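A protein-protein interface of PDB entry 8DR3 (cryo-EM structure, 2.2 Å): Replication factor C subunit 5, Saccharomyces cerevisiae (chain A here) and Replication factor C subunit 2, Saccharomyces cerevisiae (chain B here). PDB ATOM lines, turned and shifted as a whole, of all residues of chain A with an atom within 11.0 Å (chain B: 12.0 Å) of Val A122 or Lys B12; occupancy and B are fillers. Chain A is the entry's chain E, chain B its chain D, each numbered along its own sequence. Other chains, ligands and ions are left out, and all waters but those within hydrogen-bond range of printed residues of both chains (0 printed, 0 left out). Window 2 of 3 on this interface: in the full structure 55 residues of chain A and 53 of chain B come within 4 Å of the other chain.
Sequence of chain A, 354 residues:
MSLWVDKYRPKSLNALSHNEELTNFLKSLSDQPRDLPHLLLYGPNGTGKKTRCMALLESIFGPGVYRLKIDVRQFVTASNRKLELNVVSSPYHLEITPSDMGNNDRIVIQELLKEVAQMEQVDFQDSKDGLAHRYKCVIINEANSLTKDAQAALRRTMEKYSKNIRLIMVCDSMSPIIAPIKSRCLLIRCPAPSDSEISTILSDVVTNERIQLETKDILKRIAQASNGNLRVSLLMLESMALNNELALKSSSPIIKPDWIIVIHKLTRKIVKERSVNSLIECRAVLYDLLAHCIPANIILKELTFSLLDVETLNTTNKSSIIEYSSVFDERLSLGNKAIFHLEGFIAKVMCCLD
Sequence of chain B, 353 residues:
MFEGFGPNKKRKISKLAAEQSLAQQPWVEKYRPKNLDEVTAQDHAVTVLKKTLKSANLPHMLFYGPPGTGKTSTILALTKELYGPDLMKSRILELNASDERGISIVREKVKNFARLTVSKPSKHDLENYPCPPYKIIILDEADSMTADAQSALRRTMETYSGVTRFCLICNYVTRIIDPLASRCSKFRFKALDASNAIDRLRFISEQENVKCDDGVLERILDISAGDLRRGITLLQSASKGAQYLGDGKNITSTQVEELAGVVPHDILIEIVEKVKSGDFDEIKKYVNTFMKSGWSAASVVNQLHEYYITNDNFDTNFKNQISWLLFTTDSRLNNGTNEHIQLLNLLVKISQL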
ATOM      1  N   ARG A  34      23.503  30.148  11.787  1.00  0.00           N
ATOM      2  CA  ARG A  34      24.787  29.488  11.569  1.00  0.00           C
ATOM      3  C   ARG A  34      25.584  29.377  12.864  1.00  0.00           C
ATOM      4  O   ARG A  34      26.202  28.341  13.132  1.00  0.00           O
ATOM      5  CB  ARG A  34      25.588  30.237  10.506  1.00  0.00           C
ATOM      6  CG  ARG A  34      24.978  30.151   9.114  1.00  0.00           C
ATOM      7  CD  ARG A  34      26.034  30.016   8.028  1.00  0.00           C
ATOM      8  NE  ARG A  34      26.185  28.633   7.590  1.00  0.00           N
ATOM      9  CZ  ARG A  34      25.481  28.067   6.619  1.00  0.00           C
ATOM     10  NH1 ARG A  34      24.554  28.737   5.953  1.00  0.00           N
ATOM     11  NH2 ARG A  34      25.710  26.795   6.310  1.00  0.00           N
ATOM     12  N   PRO A  91      15.383  14.026   8.617  1.00  0.00           N
ATOM     13  CA  PRO A  91      16.570  14.267   7.781  1.00  0.00           C
ATOM     14  C   PRO A  91      17.488  15.346   8.327  1.00  0.00           C
ATOM     15  O   PRO A  91      18.655  15.405   7.920  1.00  0.00           O
ATOM     16  CB  PRO A  91      15.977  14.665   6.419  1.00  0.00           C
ATOM     17  CG  PRO A  91      14.533  14.941   6.663  1.00  0.00           C
ATOM     18  CD  PRO A  91      14.133  14.134   7.848  1.00  0.00           C
ATOM     19  N   TYR A  92      17.008  16.200   9.235  1.00  0.00           N
ATOM     20  CA  TYR A  92      17.807  17.295   9.765  1.00  0.00           C
ATOM     21  C   TYR A  92      18.087  17.211  11.260  1.00  0.00           C
ATOM     22  O   TYR A  92      19.067  17.812  11.712  1.00  0.00           O
ATOM     23  CB  TYR A  92      17.122  18.641   9.477  1.00  0.00           C
ATOM     24  CG  TYR A  92      16.560  18.755   8.077  1.00  0.00           C
ATOM     25  CD1 TYR A  92      17.386  19.033   6.996  1.00  0.00           C
ATOM     26  CD2 TYR A  92      15.204  18.586   7.837  1.00  0.00           C
ATOM     27  CE1 TYR A  92      16.876  19.138   5.714  1.00  0.00           C
ATOM     28  CE2 TYR A  92      14.685  18.689   6.560  1.00  0.00           C
ATOM     29  CZ  TYR A  92      15.525  18.966   5.503  1.00  0.00           C
ATOM     30  OH  TYR A  92      15.010  19.068   4.231  1.00  0.00           O
ATOM     31  N   VAL A 116      27.388  10.503  17.047  1.00  0.00           N
ATOM     32  CA  VAL A 116      26.785  11.512  16.181  1.00  0.00           C
ATOM     33  C   VAL A 116      27.647  12.768  16.147  1.00  0.00           C
ATOM     34  O   VAL A 116      27.742  13.438  15.111  1.00  0.00           O
ATOM     35  CB  VAL A 116      25.351  11.824  16.643  1.00  0.00           C
ATOM     36  CG1 VAL A 116      24.770  12.981  15.842  1.00  0.00           C
ATOM     37  CG2 VAL A 116      24.474  10.588  16.517  1.00  0.00           C
ATOM     38  N   GLN A 118      30.899  13.099  16.313  1.00  0.00           N
ATOM     39  CA  GLN A 118      32.138  12.961  15.559  1.00  0.00           C
ATOM     40  C   GLN A 118      31.913  12.843  14.058  1.00  0.00           C
ATOM     41  O   GLN A 118      32.892  12.770  13.308  1.00  0.00           O
ATOM     42  CB  GLN A 118      32.916  11.741  16.057  1.00  0.00           C
ATOM     43  CG  GLN A 118      33.514  11.916  17.444  1.00  0.00           C
ATOM     44  CD  GLN A 118      33.969  10.604  18.053  1.00  0.00           C
ATOM     45  OE1 GLN A 118      33.954   9.564  17.397  1.00  0.00           O
ATOM     46  NE2 GLN A 118      34.379  10.649  19.315  1.00  0.00           N
ATOM     47  N   MET A 119      30.664  12.824  13.601  1.00  0.00           N
ATOM     48  CA  MET A 119      30.344  12.693  12.186  1.00  0.00           C
ATOM     49  C   MET A 119      29.994  14.067  11.629  1.00  0.00           C
ATOM     50  O   MET A 119      29.102  14.744  12.151  1.00  0.00           O
ATOM     51  CB  MET A 119      29.187  11.718  11.980  1.00  0.00           C
ATOM     52  CG  MET A 119      28.876  11.433  10.516  1.00  0.00           C
ATOM     53  SD  MET A 119      27.781  10.024  10.204  1.00  0.00           S
ATOM     54  CE  MET A 119      27.332   9.485  11.855  1.00  0.00           C
ATOM     55  N   GLU A 120      30.694  14.472  10.573  1.00  0.00           N
ATOM     56  CA  GLU A 120      30.434  15.755   9.944  1.00  0.00           C
ATOM     57  C   GLU A 120      29.257  15.648   8.978  1.00  0.00           C
ATOM     58  O   GLU A 120      28.851  14.559   8.566  1.00  0.00           O
ATOM     59  CB  GLU A 120      31.676  16.251   9.203  1.00  0.00           C
ATOM     60  CG  GLU A 120      32.860  16.542  10.112  1.00  0.00           C
ATOM     61  CD  GLU A 120      33.981  17.271   9.398  1.00  0.00           C
ATOM     62  OE1 GLU A 120      33.766  17.721   8.253  1.00  0.00           O
ATOM     63  OE2 GLU A 120      35.078  17.394   9.983  1.00  0.00           O
ATOM     64  N   GLN A 121      28.708  16.806   8.621  1.00  0.00           N
ATOM     65  CA  GLN A 121      27.579  16.880   7.701  1.00  0.00           C
ATOM     66  C   GLN A 121      28.102  16.976   6.273  1.00  0.00           C
ATOM     67  O   GLN A 121      28.883  17.879   5.951  1.00  0.00           O
ATOM     68  CB  GLN A 121      26.694  18.081   8.032  1.00  0.00           C
ATOM     69  CG  GLN A 121      25.527  18.270   7.073  1.00  0.00           C
ATOM     70  CD  GLN A 121      24.392  19.071   7.681  1.00  0.00           C
ATOM     71  OE1 GLN A 121      24.410  19.395   8.867  1.00  0.00           O
ATOM     72  NE2 GLN A 121      23.396  19.398   6.865  1.00  0.00           N
ATOM     73  N   VAL A 122      27.672  16.047   5.422  1.00  0.00           N
ATOM     74  CA  VAL A 122      28.103  16.022   4.031  1.00  0.00           C
ATOM     75  C   VAL A 122      26.946  16.132   3.048  1.00  0.00           C
ATOM     76  O   VAL A 122      27.173  16.529   1.893  1.00  0.00           O
ATOM     77  CB  VAL A 122      28.930  14.753   3.733  1.00  0.00           C
ATOM     78  CG1 VAL A 122      29.986  14.541   4.809  1.00  0.00           C
ATOM     79  CG2 VAL A 122      28.022  13.537   3.622  1.00  0.00           C
ATOM     80  N   ASP A 123      25.719  15.802   3.443  1.00  0.00           N
ATOM     81  CA  ASP A 123      24.586  15.924   2.538  1.00  0.00           C
ATOM     82  C   ASP A 123      24.321  17.390   2.218  1.00  0.00           C
ATOM     83  O   ASP A 123      24.367  18.254   3.098  1.00  0.00           O
ATOM     84  CB  ASP A 123      23.342  15.286   3.156  1.00  0.00           C
ATOM     85  CG  ASP A 123      23.511  13.800   3.403  1.00  0.00           C
ATOM     86  OD1 ASP A 123      24.655  13.309   3.316  1.00  0.00           O
ATOM     87  OD2 ASP A 123      22.499  13.124   3.684  1.00  0.00           O
ATOM     88  N   PHE A 124      24.034  17.667   0.947  1.00  0.00           N
ATOM     89  CA  PHE A 124      23.816  19.037   0.499  1.00  0.00           C
ATOM     90  C   PHE A 124      22.450  19.542   0.948  1.00  0.00           C
ATOM     91  O   PHE A 124      21.468  19.441   0.206  1.00  0.00           O
ATOM     92  CB  PHE A 124      23.942  19.130  -1.023  1.00  0.00           C
ATOM     93  CG  PHE A 124      23.982  20.540  -1.541  1.00  0.00           C
ATOM     94  CD1 PHE A 124      25.013  21.393  -1.187  1.00  0.00           C
ATOM     95  CD2 PHE A 124      22.987  21.012  -2.381  1.00  0.00           C
ATOM     96  CE1 PHE A 124      25.052  22.691  -1.661  1.00  0.00           C
ATOM     97  CE2 PHE A 124      23.021  22.309  -2.859  1.00  0.00           C
ATOM     98  CZ  PHE A 124      24.056  23.149  -2.497  1.00  0.00           C
ATOM     99  N   GLN A 125      22.382  20.087   2.163  1.00  0.00           N
ATOM    100  CA  GLN A 125      21.145  20.641   2.710  1.00  0.00           C
ATOM    101  C   GLN A 125      21.191  22.156   2.538  1.00  0.00           C
ATOM    102  O   GLN A 125      21.542  22.908   3.448  1.00  0.00           O
ATOM    103  CB  GLN A 125      20.978  20.236   4.170  1.00  0.00           C
ATOM    104  CG  GLN A 125      20.829  18.737   4.382  1.00  0.00           C
ATOM    105  CD  GLN A 125      20.537  18.378   5.825  1.00  0.00           C
ATOM    106  OE1 GLN A 125      20.919  19.099   6.747  1.00  0.00           O
ATOM    107  NE2 GLN A 125      19.857  17.256   6.030  1.00  0.00           N
ATOM    108  N   ASP A 126      20.825  22.605   1.339  1.00  0.00           N
ATOM    109  CA  ASP A 126      20.872  24.026   1.026  1.00  0.00           C
ATOM    110  C   ASP A 126      19.989  24.815   1.984  1.00  0.00           C
ATOM    111  O   ASP A 126      18.853  24.429   2.274  1.00  0.00           O
ATOM    112  CB  ASP A 126      20.426  24.263  -0.418  1.00  0.00           C
ATOM    113  CG  ASP A 126      20.697  25.681  -0.886  1.00  0.00           C
ATOM    114  OD1 ASP A 126      21.336  26.446  -0.134  1.00  0.00           O
ATOM    115  OD2 ASP A 126      20.269  26.029  -2.006  1.00  0.00           O
ATOM    116  N   LEU A 131      24.314  28.533   0.997  1.00  0.00           N
ATOM    117  CA  LEU A 131      25.192  27.395   1.208  1.00  0.00           C
ATOM    118  C   LEU A 131      24.406  26.265   1.873  1.00  0.00           C
ATOM    119  O   LEU A 131      23.181  26.324   2.004  1.00  0.00           O
ATOM    120  CB  LEU A 131      26.406  27.813   2.036  1.00  0.00           C
ATOM    121  CG  LEU A 131      27.017  29.172   1.685  1.00  0.00           C
ATOM    122  CD1 LEU A 131      28.210  29.468   2.580  1.00  0.00           C
ATOM    123  CD2 LEU A 131      27.420  29.220   0.218  1.00  0.00           C
ATOM    124  N   ALA A 132      25.109  25.222   2.303  1.00  0.00           N
ATOM    125  CA  ALA A 132      24.489  24.057   2.916  1.00  0.00           C
ATOM    126  C   ALA A 132      24.658  24.098   4.430  1.00  0.00           C
ATOM    127  O   ALA A 132      25.633  24.644   4.952  1.00  0.00           O
ATOM    128  CB  ALA A 132      25.093  22.766   2.362  1.00  0.00           C
ATOM    129  N   HIS A 133      23.689  23.515   5.131  1.00  0.00           N
ATOM    130  CA  HIS A 133      23.761  23.447   6.584  1.00  0.00           C
ATOM    131  C   HIS A 133      24.967  22.620   7.011  1.00  0.00           C
ATOM    132  O   HIS A 133      25.308  21.617   6.381  1.00  0.00           O
ATOM    133  CB  HIS A 133      22.476  22.842   7.150  1.00  0.00           C
ATOM    134  CG  HIS A 133      21.266  23.700   6.948  1.00  0.00           C
ATOM    135  ND1 HIS A 133      20.213  23.325   6.143  1.00  0.00           N
ATOM    136  CD2 HIS A 133      20.943  24.917   7.446  1.00  0.00           C
ATOM    137  CE1 HIS A 133      19.293  24.272   6.153  1.00  0.00           C
ATOM    138  NE2 HIS A 133      19.712  25.250   6.937  1.00  0.00           N
ATOM    139  N   ARG A 134      25.613  23.050   8.094  1.00  0.00           N
ATOM    140  CA  ARG A 134      26.848  22.433   8.552  1.00  0.00           C
ATOM    141  C   ARG A 134      26.694  21.620   9.828  1.00  0.00           C
ATOM    142  O   ARG A 134      27.609  20.863  10.169  1.00  0.00           O
ATOM    143  CB  ARG A 134      27.923  23.509   8.774  1.00  0.00           C
ATOM    144  CG  ARG A 134      28.497  24.094   7.491  1.00  0.00           C
ATOM    145  CD  ARG A 134      29.374  23.094   6.753  1.00  0.00           C
ATOM    146  NE  ARG A 134      29.829  23.611   5.468  1.00  0.00           N
ATOM    147  CZ  ARG A 134      30.713  23.006   4.687  1.00  0.00           C
ATOM    148  NH1 ARG A 134      31.263  21.851   5.029  1.00  0.00           N
ATOM    149  NH2 ARG A 134      31.058  23.575   3.535  1.00  0.00           N
ATOM    150  N   TYR A 135      25.575  21.745  10.539  1.00  0.00           N
ATOM    151  CA  TYR A 135      25.374  21.034  11.791  1.00  0.00           C
ATOM    152  C   TYR A 135      23.992  20.400  11.825  1.00  0.00           C
ATOM    153  O   TYR A 135      23.060  20.861  11.161  1.00  0.00           O
ATOM    154  CB  TYR A 135      25.547  21.966  13.006  1.00  0.00           C
ATOM    155  CG  TYR A 135      24.546  23.101  13.078  1.00  0.00           C
ATOM    156  CD1 TYR A 135      23.262  22.894  13.570  1.00  0.00           C
ATOM    157  CD2 TYR A 135      24.889  24.381  12.666  1.00  0.00           C
ATOM    158  CE1 TYR A 135      22.349  23.928  13.640  1.00  0.00           C
ATOM    159  CE2 TYR A 135      23.982  25.421  12.735  1.00  0.00           C
ATOM    160  CZ  TYR A 135      22.714  25.188  13.223  1.00  0.00           C
ATOM    161  OH  TYR A 135      21.808  26.221  13.292  1.00  0.00           O
ATOM    162  N   LYS A 136      23.876  19.334  12.608  1.00  0.00           N
ATOM    163  CA  LYS A 136      22.606  18.694  12.910  1.00  0.00           C
ATOM    164  C   LYS A 136      22.147  19.090  14.307  1.00  0.00           C
ATOM    165  O   LYS A 136      22.947  19.454  15.171  1.00  0.00           O
ATOM    166  CB  LYS A 136      22.725  17.171  12.811  1.00  0.00           C
ATOM    167  CG  LYS A 136      22.310  16.600  11.464  1.00  0.00           C
ATOM    168  CD  LYS A 136      22.877  15.202  11.246  1.00  0.00           C
ATOM    169  CE  LYS A 136      21.946  14.125  11.782  1.00  0.00           C
ATOM    170  NZ  LYS A 136      22.000  14.021  13.266  1.00  0.00           N
ATOM    171  N   LYS A 163      30.874  22.334  16.342  1.00  0.00           N
ATOM    172  CA  LYS A 163      30.844  22.603  14.911  1.00  0.00           C
ATOM    173  C   LYS A 163      30.009  21.576  14.154  1.00  0.00           C
ATOM    174  O   LYS A 163      29.530  21.876  13.056  1.00  0.00           O
ATOM    175  CB  LYS A 163      32.284  22.653  14.379  1.00  0.00           C
ATOM    176  CG  LYS A 163      32.491  22.191  12.931  1.00  0.00           C
ATOM    177  CD  LYS A 163      32.911  20.723  12.814  1.00  0.00           C
ATOM    178  CE  LYS A 163      34.244  20.419  13.497  1.00  0.00           C
ATOM    179  NZ  LYS A 163      34.564  18.965  13.464  1.00  0.00           N
ATOM    180  N   ASN A 164      29.801  20.388  14.722  1.00  0.00           N
ATOM    181  CA  ASN A 164      29.051  19.333  14.052  1.00  0.00           C
ATOM    182  C   ASN A 164      27.599  19.235  14.500  1.00  0.00           C
ATOM    183  O   ASN A 164      26.737  18.912  13.678  1.00  0.00           O
ATOM    184  CB  ASN A 164      29.727  17.977  14.278  1.00  0.00           C
ATOM    185  CG  ASN A 164      30.948  17.781  13.404  1.00  0.00           C
ATOM    186  OD1 ASN A 164      31.000  18.265  12.275  1.00  0.00           O
ATOM    187  ND2 ASN A 164      31.938  17.063  13.923  1.00  0.00           N
ATOM    188  N   ILE A 165      27.302  19.492  15.775  1.00  0.00           N
ATOM    189  CA  ILE A 165      25.947  19.361  16.293  1.00  0.00           C
ATOM    190  C   ILE A 165      25.611  20.568  17.156  1.00  0.00           C
ATOM    191  O   ILE A 165      26.488  21.271  17.660  1.00  0.00           O
ATOM    192  CB  ILE A 165      25.751  18.068  17.110  1.00  0.00           C
ATOM    193  CG1 ILE A 165      26.633  18.100  18.363  1.00  0.00           C
ATOM    194  CG2 ILE A 165      26.053  16.849  16.247  1.00  0.00           C
ATOM    195  CD1 ILE A 165      26.810  16.763  19.038  1.00  0.00           C
ATOM    196  N   ARG B  11      25.117  12.983  -1.777  1.00  0.00           N
ATOM    197  CA  ARG B  11      25.933  14.110  -2.210  1.00  0.00           C
ATOM    198  C   ARG B  11      27.094  14.339  -1.248  1.00  0.00           C
ATOM    199  O   ARG B  11      27.315  13.551  -0.330  1.00  0.00           O
ATOM    200  CB  ARG B  11      25.082  15.377  -2.318  1.00  0.00           C
ATOM    201  N   LYS B  12      27.833  15.424  -1.467  1.00  0.00           N
ATOM    202  CA  LYS B  12      28.968  15.760  -0.621  1.00  0.00           C
ATOM    203  C   LYS B  12      29.143  17.272  -0.609  1.00  0.00           C
ATOM    204  O   LYS B  12      28.684  17.978  -1.510  1.00  0.00           O
ATOM    205  CB  LYS B  12      30.252  15.074  -1.105  1.00  0.00           C
ATOM    206  CG  LYS B  12      31.264  14.803  -0.003  1.00  0.00           C
ATOM    207  CD  LYS B  12      31.002  13.468   0.676  1.00  0.00           C
ATOM    208  CE  LYS B  12      31.944  13.249   1.850  1.00  0.00           C
ATOM    209  NZ  LYS B  12      31.751  11.915   2.480  1.00  0.00           N
ATOM    210  N   ILE B  13      29.818  17.760   0.430  1.00  0.00           N
ATOM    211  CA  ILE B  13      30.074  19.183   0.613  1.00  0.00           C
ATOM    212  C   ILE B  13      31.568  19.385   0.814  1.00  0.00           C
ATOM    213  O   ILE B  13      32.206  18.652   1.578  1.00  0.00           O
ATOM    214  CB  ILE B  13      29.287  19.760   1.808  1.00  0.00           C
ATOM    215  CG1 ILE B  13      27.784  19.729   1.525  1.00  0.00           C
ATOM    216  CG2 ILE B  13      29.745  21.182   2.102  1.00  0.00           C
ATOM    217  CD1 ILE B  13      26.926  19.894   2.764  1.00  0.00           C
ATOM    218  N   SER B  14      32.125  20.380   0.126  1.00  0.00           N
ATOM    219  CA  SER B  14      33.532  20.708   0.302  1.00  0.00           C
ATOM    220  C   SER B  14      33.798  21.127   1.743  1.00  0.00           C
ATOM    221  O   SER B  14      33.038  21.895   2.337  1.00  0.00           O
ATOM    222  CB  SER B  14      33.937  21.828  -0.657  1.00  0.00           C
ATOM    223  OG  SER B  14      33.038  22.920  -0.573  1.00  0.00           O
ATOM    224  N   LYS B  15      34.890  20.614   2.306  1.00  0.00           N
ATOM    225  CA  LYS B  15      35.230  20.923   3.687  1.00  0.00           C
ATOM    226  C   LYS B  15      35.584  22.397   3.834  1.00  0.00           C
ATOM    227  O   LYS B  15      36.189  23.001   2.944  1.00  0.00           O
ATOM    228  CB  LYS B  15      36.397  20.053   4.158  1.00  0.00           C
ATOM    229  CG  LYS B  15      36.197  18.561   3.935  1.00  0.00           C
ATOM    230  CD  LYS B  15      37.489  17.791   4.151  1.00  0.00           C
ATOM    231  CE  LYS B  15      37.234  16.297   4.265  1.00  0.00           C
ATOM    232  NZ  LYS B  15      38.499  15.516   4.330  1.00  0.00           N
ATOM    233  N   LEU B  16      35.202  22.973   4.968  1.00  0.00           N
ATOM    234  CA  LEU B  16      35.449  24.379   5.248  1.00  0.00           C
ATOM    235  C   LEU B  16      36.835  24.573   5.848  1.00  0.00           C
ATOM    236  O   LEU B  16      37.381  23.685   6.508  1.00  0.00           O
ATOM    237  CB  LEU B  16      34.394  24.930   6.208  1.00  0.00           C
ATOM    238  CG  LEU B  16      33.155  25.552   5.563  1.00  0.00           C
ATOM    239  CD1 LEU B  16      32.004  25.556   6.551  1.00  0.00           C
ATOM    240  CD2 LEU B  16      33.450  26.959   5.069  1.00  0.00           C
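O of Arg B11 touches O of Val A122, 3.7 Å away. Lys B12 touches Val A122 (CA to O, 3.2 Å). O of Asp A123 touches CD1 of Ile B13, 3.1 Å away. Phe A124 touches Ile B13. Ile B13 touches Ala A132 (CD1 to CB, 3.4 Å). NH2 of Arg A134 touches CG2 of Ile B13, 3.1 Å away. NE of Arg A134 touches CD1 of Leu B16 (3.1 Å).
Hydrophobic or aromatic side chains of chain A within 4 Å of the printed part of chain B: Val A122 and Ala A132. Of the 6 printed residues of chain B, 5 touch a printed residue of chain A. Hydrophobic or aromatic side chains of chain B that line the printed part of chain A: Ile B13 and Leu B16. Among the printed residues, 9 pairs touch across the chains.
O of Ala A132 lies within hydrogen-bond range of NH2 of Arg A34, at 2.5 Å.
The backbone carbonyl oxygen of Val A122 sits at hydrogen-bond distance from the backbone NH of Ile B13. The backbone carbonyl oxygen (O) of Ser B14 lies within hydrogen-bond range of the guanidinium group (NH2) of Arg A134, at 2.9 Å.
Printed residues of chain B within 4 Å of Val A122: Arg B11 (3.7 Å), Lys B12 (3.2 Å) and Ile B13 (3.3 Å). Asp A123 touches one residue of chain B. Of chain B, only Ile B13 comes within 4 Å of Phe A124. Printed residues of chain B within 4 Å of Ala A132: Ile B13 (3.4 Å). Of the printed residues of chain B, Arg A134 touches Ile B13 (3.1 Å), Ser B14 (2.9 Å) and Leu B16 (3.1 Å). Of the printed residues of chain A, Lys B12 touches Val A122. Of chain A, only Val A122 (3.3 Å), Asp A123 (3.1 Å), Phe A124 (3.9 Å), Ala A132 (3.4 Å) and Arg A134 (3.1 Å) come within 4 Å of Ile B13. Of chain A, only Arg A134 (2.9 Å) comes within 4 Å of Ser B14. The nearest residue of chain B that does not touch Val A122 is Ser B14 (6.5 Å). The nearest printed residue of chain A that does not touch Leu B16 is Leu A131 (6.3 Å).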
